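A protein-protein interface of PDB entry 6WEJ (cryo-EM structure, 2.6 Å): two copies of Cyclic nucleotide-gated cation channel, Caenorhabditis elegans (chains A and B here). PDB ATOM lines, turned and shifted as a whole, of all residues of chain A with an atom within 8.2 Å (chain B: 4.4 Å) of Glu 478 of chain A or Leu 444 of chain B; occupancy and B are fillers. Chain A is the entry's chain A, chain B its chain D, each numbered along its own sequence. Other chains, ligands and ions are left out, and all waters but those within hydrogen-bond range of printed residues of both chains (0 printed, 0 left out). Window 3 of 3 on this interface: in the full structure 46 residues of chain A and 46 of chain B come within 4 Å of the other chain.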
ATOM      1  N   VAL A 467      11.532  13.055   6.028  1.00  0.00           N
ATOM      2  CA  VAL A 467      12.220  14.304   5.729  1.00  0.00           C
ATOM      3  C   VAL A 467      11.774  14.845   4.380  1.00  0.00           C
ATOM      4  O   VAL A 467      11.536  16.050   4.228  1.00  0.00           O
ATOM      5  CB  VAL A 467      13.745  14.086   5.784  1.00  0.00           C
ATOM      6  CG1 VAL A 467      14.474  15.187   5.060  1.00  0.00           C
ATOM      7  CG2 VAL A 467      14.208  14.015   7.219  1.00  0.00           C
ATOM      8  N   LEU A 471       9.105  18.233   5.538  1.00  0.00           N
ATOM      9  CA  LEU A 471       9.938  19.393   5.802  1.00  0.00           C
ATOM     10  C   LEU A 471      10.066  20.260   4.564  1.00  0.00           C
ATOM     11  O   LEU A 471       9.888  19.789   3.437  1.00  0.00           O
ATOM     12  CB  LEU A 471      11.328  18.952   6.261  1.00  0.00           C
ATOM     13  CG  LEU A 471      11.432  18.354   7.657  1.00  0.00           C
ATOM     14  CD1 LEU A 471      12.872  18.002   7.937  1.00  0.00           C
ATOM     15  CD2 LEU A 471      10.914  19.328   8.687  1.00  0.00           C
ATOM     16  N   PRO A 472      10.366  21.543   4.734  1.00  0.00           N
ATOM     17  CA  PRO A 472      10.622  22.400   3.579  1.00  0.00           C
ATOM     18  C   PRO A 472      12.005  22.159   3.001  1.00  0.00           C
ATOM     19  O   PRO A 472      12.910  21.669   3.677  1.00  0.00           O
ATOM     20  CB  PRO A 472      10.499  23.811   4.157  1.00  0.00           C
ATOM     21  CG  PRO A 472      10.825  23.656   5.582  1.00  0.00           C
ATOM     22  CD  PRO A 472      10.324  22.310   5.987  1.00  0.00           C
ATOM     23  N   ASP A 473      12.160  22.528   1.726  1.00  0.00           N
ATOM     24  CA  ASP A 473      13.403  22.265   1.011  1.00  0.00           C
ATOM     25  C   ASP A 473      14.615  22.828   1.739  1.00  0.00           C
ATOM     26  O   ASP A 473      15.716  22.284   1.617  1.00  0.00           O
ATOM     27  CB  ASP A 473      13.330  22.843  -0.400  1.00  0.00           C
ATOM     28  CG  ASP A 473      12.158  22.304  -1.188  1.00  0.00           C
ATOM     29  OD1 ASP A 473      11.347  21.559  -0.606  1.00  0.00           O
ATOM     30  OD2 ASP A 473      12.050  22.626  -2.389  1.00  0.00           O
ATOM     31  N   LYS A 474      14.436  23.904   2.500  1.00  0.00           N
ATOM     32  CA  LYS A 474      15.549  24.471   3.254  1.00  0.00           C
ATOM     33  C   LYS A 474      16.028  23.500   4.323  1.00  0.00           C
ATOM     34  O   LYS A 474      17.224  23.199   4.416  1.00  0.00           O
ATOM     35  CB  LYS A 474      15.126  25.802   3.875  1.00  0.00           C
ATOM     36  CG  LYS A 474      16.261  26.615   4.451  1.00  0.00           C
ATOM     37  CD  LYS A 474      17.147  27.155   3.354  1.00  0.00           C
ATOM     38  CE  LYS A 474      18.301  27.948   3.925  1.00  0.00           C
ATOM     39  NZ  LYS A 474      19.167  28.493   2.850  1.00  0.00           N
ATOM     40  N   LEU A 475      15.103  22.988   5.135  1.00  0.00           N
ATOM     41  CA  LEU A 475      15.482  22.060   6.192  1.00  0.00           C
ATOM     42  C   LEU A 475      15.964  20.736   5.619  1.00  0.00           C
ATOM     43  O   LEU A 475      16.893  20.126   6.156  1.00  0.00           O
ATOM     44  CB  LEU A 475      14.310  21.832   7.141  1.00  0.00           C
ATOM     45  CG  LEU A 475      14.069  22.914   8.185  1.00  0.00           C
ATOM     46  CD1 LEU A 475      12.903  22.530   9.064  1.00  0.00           C
ATOM     47  CD2 LEU A 475      15.317  23.116   9.013  1.00  0.00           C
ATOM     48  N   GLN A 476      15.342  20.274   4.534  1.00  0.00           N
ATOM     49  CA  GLN A 476      15.793  19.045   3.892  1.00  0.00           C
ATOM     50  C   GLN A 476      17.221  19.188   3.389  1.00  0.00           C
ATOM     51  O   GLN A 476      18.054  18.299   3.589  1.00  0.00           O
ATOM     52  CB  GLN A 476      14.859  18.682   2.745  1.00  0.00           C
ATOM     53  CG  GLN A 476      13.437  18.438   3.177  1.00  0.00           C
ATOM     54  CD  GLN A 476      12.545  18.083   2.021  1.00  0.00           C
ATOM     55  OE1 GLN A 476      13.007  17.902   0.897  1.00  0.00           O
ATOM     56  NE2 GLN A 476      11.251  17.981   2.286  1.00  0.00           N
ATOM     57  N   ALA A 477      17.522  20.311   2.737  1.00  0.00           N
ATOM     58  CA  ALA A 477      18.872  20.525   2.237  1.00  0.00           C
ATOM     59  C   ALA A 477      19.870  20.649   3.376  1.00  0.00           C
ATOM     60  O   ALA A 477      20.979  20.121   3.289  1.00  0.00           O
ATOM     61  CB  ALA A 477      18.913  21.765   1.349  1.00  0.00           C
ATOM     62  N   GLU A 478      19.495  21.325   4.461  1.00  0.00           N
ATOM     63  CA  GLU A 478      20.421  21.459   5.581  1.00  0.00           C
ATOM     64  C   GLU A 478      20.689  20.114   6.245  1.00  0.00           C
ATOM     65  O   GLU A 478      21.834  19.807   6.600  1.00  0.00           O
ATOM     66  CB  GLU A 478      19.885  22.466   6.594  1.00  0.00           C
ATOM     67  CG  GLU A 478      19.888  23.893   6.082  1.00  0.00           C
ATOM     68  CD  GLU A 478      19.579  24.905   7.162  1.00  0.00           C
ATOM     69  OE1 GLU A 478      19.312  24.492   8.308  1.00  0.00           O
ATOM     70  OE2 GLU A 478      19.605  26.117   6.867  1.00  0.00           O
ATOM     71  N   ILE A 479      19.654  19.292   6.408  1.00  0.00           N
ATOM     72  CA  ILE A 479      19.846  17.977   7.009  1.00  0.00           C
ATOM     73  C   ILE A 479      20.700  17.096   6.109  1.00  0.00           C
ATOM     74  O   ILE A 479      21.615  16.412   6.580  1.00  0.00           O
ATOM     75  CB  ILE A 479      18.490  17.324   7.317  1.00  0.00           C
ATOM     76  CG1 ILE A 479      17.793  18.062   8.455  1.00  0.00           C
ATOM     77  CG2 ILE A 479      18.675  15.872   7.685  1.00  0.00           C
ATOM     78  CD1 ILE A 479      16.447  17.498   8.801  1.00  0.00           C
ATOM     79  N   ALA A 480      20.426  17.095   4.803  1.00  0.00           N
ATOM     80  CA  ALA A 480      21.221  16.282   3.889  1.00  0.00           C
ATOM     81  C   ALA A 480      22.664  16.757   3.839  1.00  0.00           C
ATOM     82  O   ALA A 480      23.585  15.948   3.690  1.00  0.00           O
ATOM     83  CB  ALA A 480      20.602  16.301   2.493  1.00  0.00           C
ATOM     84  N   MET A 481      22.884  18.066   3.956  1.00  0.00           N
ATOM     85  CA  MET A 481      24.242  18.593   3.976  1.00  0.00           C
ATOM     86  C   MET A 481      24.967  18.178   5.243  1.00  0.00           C
ATOM     87  O   MET A 481      26.168  17.895   5.218  1.00  0.00           O
ATOM     88  CB  MET A 481      24.215  20.114   3.853  1.00  0.00           C
ATOM     89  CG  MET A 481      24.006  20.624   2.449  1.00  0.00           C
ATOM     90  SD  MET A 481      25.521  20.571   1.489  1.00  0.00           S
ATOM     91  CE  MET A 481      26.564  21.632   2.482  1.00  0.00           C
ATOM     92  N   GLN A 482      24.257  18.146   6.367  1.00  0.00           N
ATOM     93  CA  GLN A 482      24.906  17.753   7.609  1.00  0.00           C
ATOM     94  C   GLN A 482      25.312  16.287   7.577  1.00  0.00           C
ATOM     95  O   GLN A 482      26.377  15.918   8.088  1.00  0.00           O
ATOM     96  CB  GLN A 482      23.987  18.033   8.790  1.00  0.00           C
ATOM     97  CG  GLN A 482      24.729  18.354  10.061  1.00  0.00           C
ATOM     98  CD  GLN A 482      23.901  19.175  11.011  1.00  0.00           C
ATOM     99  OE1 GLN A 482      24.131  20.371  11.186  1.00  0.00           O
ATOM    100  NE2 GLN A 482      22.925  18.540  11.636  1.00  0.00           N
ATOM    101  N   VAL A 483      24.482  15.435   6.975  1.00  0.00           N
ATOM    102  CA  VAL A 483      24.723  13.997   7.025  1.00  0.00           C
ATOM    103  C   VAL A 483      25.762  13.569   5.995  1.00  0.00           C
ATOM    104  O   VAL A 483      26.622  12.730   6.282  1.00  0.00           O
ATOM    105  CB  VAL A 483      23.399  13.239   6.836  1.00  0.00           C
ATOM    106  CG1 VAL A 483      23.642  11.747   6.854  1.00  0.00           C
ATOM    107  CG2 VAL A 483      22.408  13.628   7.914  1.00  0.00           C
ATOM    108  N   HIS A 484      25.709  14.130   4.787  1.00  0.00           N
ATOM    109  CA  HIS A 484      26.415  13.547   3.655  1.00  0.00           C
ATOM    110  C   HIS A 484      27.563  14.372   3.096  1.00  0.00           C
ATOM    111  O   HIS A 484      28.355  13.829   2.318  1.00  0.00           O
ATOM    112  CB  HIS A 484      25.439  13.274   2.502  1.00  0.00           C
ATOM    113  CG  HIS A 484      24.331  12.331   2.846  1.00  0.00           C
ATOM    114  ND1 HIS A 484      24.489  10.965   2.843  1.00  0.00           N
ATOM    115  CD2 HIS A 484      23.040  12.560   3.184  1.00  0.00           C
ATOM    116  CE1 HIS A 484      23.350  10.391   3.177  1.00  0.00           C
ATOM    117  NE2 HIS A 484      22.453  11.337   3.388  1.00  0.00           N
ATOM    118  N   PHE A 485      27.687  15.652   3.447  1.00  0.00           N
ATOM    119  CA  PHE A 485      28.646  16.504   2.747  1.00  0.00           C
ATOM    120  C   PHE A 485      30.081  16.134   3.093  1.00  0.00           C
ATOM    121  O   PHE A 485      30.920  15.967   2.202  1.00  0.00           O
ATOM    122  CB  PHE A 485      28.388  17.973   3.064  1.00  0.00           C
ATOM    123  CG  PHE A 485      29.228  18.919   2.264  1.00  0.00           C
ATOM    124  CD1 PHE A 485      28.807  19.360   1.027  1.00  0.00           C
ATOM    125  CD2 PHE A 485      30.441  19.369   2.749  1.00  0.00           C
ATOM    126  CE1 PHE A 485      29.576  20.230   0.293  1.00  0.00           C
ATOM    127  CE2 PHE A 485      31.211  20.237   2.017  1.00  0.00           C
ATOM    128  CZ  PHE A 485      30.779  20.667   0.787  1.00  0.00           C
ATOM    129  N   VAL A 506      24.314  15.416  -2.555  1.00  0.00           N
ATOM    130  CA  VAL A 506      23.851  14.948  -1.255  1.00  0.00           C
ATOM    131  C   VAL A 506      22.341  14.987  -1.173  1.00  0.00           C
ATOM    132  O   VAL A 506      21.748  14.271  -0.360  1.00  0.00           O
ATOM    133  CB  VAL A 506      24.460  15.760  -0.087  1.00  0.00           C
ATOM    134  CG1 VAL A 506      25.967  15.754  -0.140  1.00  0.00           C
ATOM    135  CG2 VAL A 506      23.932  17.171  -0.071  1.00  0.00           C
ATOM    136  N   LEU A 507      21.690  15.810  -1.995  1.00  0.00           N
ATOM    137  CA  LEU A 507      20.236  15.722  -2.067  1.00  0.00           C
ATOM    138  C   LEU A 507      19.788  14.387  -2.654  1.00  0.00           C
ATOM    139  O   LEU A 507      18.848  13.763  -2.147  1.00  0.00           O
ATOM    140  CB  LEU A 507      19.679  16.892  -2.874  1.00  0.00           C
ATOM    141  CG  LEU A 507      19.613  18.190  -2.073  1.00  0.00           C
ATOM    142  CD1 LEU A 507      19.030  19.314  -2.902  1.00  0.00           C
ATOM    143  CD2 LEU A 507      18.794  17.969  -0.816  1.00  0.00           C
ATOM    144  N   VAL B 440      22.227  13.593  13.628  1.00  0.00           N
ATOM    145  CA  VAL B 440      22.145  14.996  13.239  1.00  0.00           C
ATOM    146  C   VAL B 440      22.485  15.877  14.436  1.00  0.00           C
ATOM    147  O   VAL B 440      22.144  15.566  15.581  1.00  0.00           O
ATOM    148  CB  VAL B 440      20.740  15.294  12.675  1.00  0.00           C
ATOM    149  CG1 VAL B 440      20.490  16.780  12.560  1.00  0.00           C
ATOM    150  CG2 VAL B 440      20.563  14.623  11.327  1.00  0.00           C
ATOM    151  N   SER B 441      23.184  16.979  14.170  1.00  0.00           N
ATOM    152  CA  SER B 441      23.559  17.916  15.221  1.00  0.00           C
ATOM    153  C   SER B 441      22.327  18.450  15.942  1.00  0.00           C
ATOM    154  O   SER B 441      21.251  18.594  15.357  1.00  0.00           O
ATOM    155  CB  SER B 441      24.357  19.076  14.632  1.00  0.00           C
ATOM    156  OG  SER B 441      24.594  20.075  15.606  1.00  0.00           O
ATOM    157  N   LYS B 442      22.495  18.758  17.230  1.00  0.00           N
ATOM    158  CA  LYS B 442      21.353  19.147  18.051  1.00  0.00           C
ATOM    159  C   LYS B 442      20.842  20.541  17.716  1.00  0.00           C
ATOM    160  O   LYS B 442      19.651  20.816  17.892  1.00  0.00           O
ATOM    161  CB  LYS B 442      21.712  19.060  19.532  1.00  0.00           C
ATOM    162  CG  LYS B 442      21.784  17.641  20.056  1.00  0.00           C
ATOM    163  CD  LYS B 442      20.481  16.901  19.805  1.00  0.00           C
ATOM    164  CE  LYS B 442      19.328  17.529  20.568  1.00  0.00           C
ATOM    165  NZ  LYS B 442      18.028  16.873  20.253  1.00  0.00           N
ATOM    166  N   GLN B 443      21.713  21.436  17.250  1.00  0.00           N
ATOM    167  CA  GLN B 443      21.247  22.755  16.841  1.00  0.00           C
ATOM    168  C   GLN B 443      20.280  22.649  15.668  1.00  0.00           C
ATOM    169  O   GLN B 443      19.224  23.294  15.653  1.00  0.00           O
ATOM    170  CB  GLN B 443      22.438  23.645  16.487  1.00  0.00           C
ATOM    171  CG  GLN B 443      22.111  25.126  16.360  1.00  0.00           C
ATOM    172  CD  GLN B 443      21.587  25.503  14.985  1.00  0.00           C
ATOM    173  OE1 GLN B 443      21.747  24.757  14.020  1.00  0.00           O
ATOM    174  NE2 GLN B 443      20.961  26.669  14.892  1.00  0.00           N
ATOM    175  N   LEU B 444      20.617  21.821  14.679  1.00  0.00           N
ATOM    176  CA  LEU B 444      19.705  21.608  13.566  1.00  0.00           C
ATOM    177  C   LEU B 444      18.416  20.946  14.024  1.00  0.00           C
ATOM    178  O   LEU B 444      17.346  21.236  13.480  1.00  0.00           O
ATOM    179  CB  LEU B 444      20.382  20.770  12.485  1.00  0.00           C
ATOM    180  CG  LEU B 444      19.633  20.692  11.159  1.00  0.00           C
ATOM    181  CD1 LEU B 444      19.356  22.083  10.646  1.00  0.00           C
ATOM    182  CD2 LEU B 444      20.434  19.904  10.146  1.00  0.00           C
ATOM    183  N   GLU B 445      18.485  20.081  15.037  1.00  0.00           N
ATOM    184  CA  GLU B 445      17.274  19.423  15.516  1.00  0.00           C
ATOM    185  C   GLU B 445      16.354  20.403  16.230  1.00  0.00           C
ATOM    186  O   GLU B 445      15.130  20.348  16.060  1.00  0.00           O
ATOM    187  CB  GLU B 445      17.633  18.263  16.437  1.00  0.00           C
ATOM    188  CG  GLU B 445      18.403  17.157  15.757  1.00  0.00           C
ATOM    189  CD  GLU B 445      18.552  15.939  16.634  1.00  0.00           C
ATOM    190  OE1 GLU B 445      17.846  15.860  17.659  1.00  0.00           O
ATOM    191  OE2 GLU B 445      19.374  15.062  16.301  1.00  0.00           O
ATOM    192  N   ILE B 446      16.915  21.311  17.027  1.00  0.00           N
ATOM    193  CA  ILE B 446      16.051  22.294  17.668  1.00  0.00           C
ATOM    194  C   ILE B 446      15.501  23.263  16.633  1.00  0.00           C
ATOM    195  O   ILE B 446      14.369  23.736  16.767  1.00  0.00           O
ATOM    196  CB  ILE B 446      16.778  23.019  18.814  1.00  0.00           C
ATOM    197  CG1 ILE B 446      17.886  23.930  18.287  1.00  0.00           C
ATOM    198  CG2 ILE B 446      17.340  22.013  19.806  1.00  0.00           C
ATOM    199  CD1 ILE B 446      18.771  24.511  19.368  1.00  0.00           C
ATOM    200  N   ARG B 447      16.256  23.544  15.567  1.00  0.00           N
ATOM    201  CA  ARG B 447      15.706  24.346  14.476  1.00  0.00           C
ATOM    202  C   ARG B 447      14.518  23.648  13.826  1.00  0.00           C
ATOM    203  O   ARG B 447      13.471  24.264  13.581  1.00  0.00           O
ATOM    204  CB  ARG B 447      16.786  24.630  13.436  1.00  0.00           C
ATOM    205  CG  ARG B 447      17.335  26.038  13.475  1.00  0.00           C
ATOM    206  CD  ARG B 447      18.386  26.233  12.404  1.00  0.00           C
ATOM    207  NE  ARG B 447      17.905  25.813  11.094  1.00  0.00           N
ATOM    208  CZ  ARG B 447      17.240  26.598  10.254  1.00  0.00           C
ATOM    209  NH1 ARG B 447      16.978  27.853  10.586  1.00  0.00           N
ATOM    210  NH2 ARG B 447      16.843  26.131   9.082  1.00  0.00           N
ATOM    211  N   VAL B 448      14.669  22.354  13.537  1.00  0.00           N
ATOM    212  CA  VAL B 448      13.601  21.590  12.903  1.00  0.00           C
ATOM    213  C   VAL B 448      12.359  21.580  13.779  1.00  0.00           C
ATOM    214  O   VAL B 448      11.238  21.796  13.300  1.00  0.00           O
ATOM    215  CB  VAL B 448      14.084  20.161  12.595  1.00  0.00           C
ATOM    216  CG1 VAL B 448      12.920  19.291  12.185  1.00  0.00           C
ATOM    217  CG2 VAL B 448      15.135  20.183  11.508  1.00  0.00           C
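The side-chain carboxylate (OE1) of Glu 478 of chain A is in salt-bridge range of the guanidinium group (NH2) of Arg 447 of chain B (3.1 Å).
N of Ser 441 of chain B sits close to NE2 of Gln 482 of chain A (3.0 Å).
Among the printed residues, merely in contact across the chains: Leu 475 of chain A with Arg 447 of chain B (3.4 Å), Leu 475 of chain A with Val 448 of chain B (3.9 Å), Glu 478 of chain A with Leu 444 of chain B (3.4 Å), Ile 479 of chain A with Leu 444 of chain B (3.6 Å), Gln 482 of chain A with Val 440 of chain B (3.1 Å) and Gln 482 of chain A with Leu 444 of chain B (3.2 Å).
Of the printed residues of chain B, Leu 475 of chain A touches Arg 447 and Val 448.
Glu 478 of chain A touches just these residues of chain B: Leu 444 and Arg 447.
Of the printed residues of chain B, Gln 482 of chain A touches Val 440 (3.1 Å), Ser 441 (3.0 Å) and Leu 444 (3.2 Å).
Of the printed residues of chain A, Val 440 of chain B touches Gln 482.
Of chain A, only Glu 478, Ile 479 and Gln 482 come within 4 Å of Leu 444 of chain B.
Of the printed residues of chain A, Arg 447 of chain B touches Leu 475 (3.4 Å) and Glu 478 (3.1 Å).
Printed residues of chain A within 4 Å of Val 448 of chain B: Leu 475.
The nearest printed residue of chain B that does not touch Glu 478 of chain A is Gln 443 of chain B (6.2 Å).
Printed residues of chain B that touch a printed residue of chain A: Val 440, Ser 441, Leu 444, Arg 447 and Val 448.
Hydrophobic or aromatic side chains of chain B within 4 Å of the printed part of chain A: Val 440, Leu 444 and Val 448.
Of the 18 printed residues of chain A, 4 touch a printed residue of chain B.
Hydrophobic or aromatic side chains of chain A within 4 Å of the printed part of chain B: Leu 475 and Ile 479.
Among the printed residues, 8 pairs touch across the chains.
Among the printed residues, Asp or Glu carboxylates within 4 Å of a Lys or Arg side-chain nitrogen of the other chain: Glu 478 of chain A with Arg 447 of chain B (3.1 Å).
No position is printed for both chains.
Of the 8 pairs that touch across the chains among the printed residues, none has its exchanged pair printed and touching as well.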
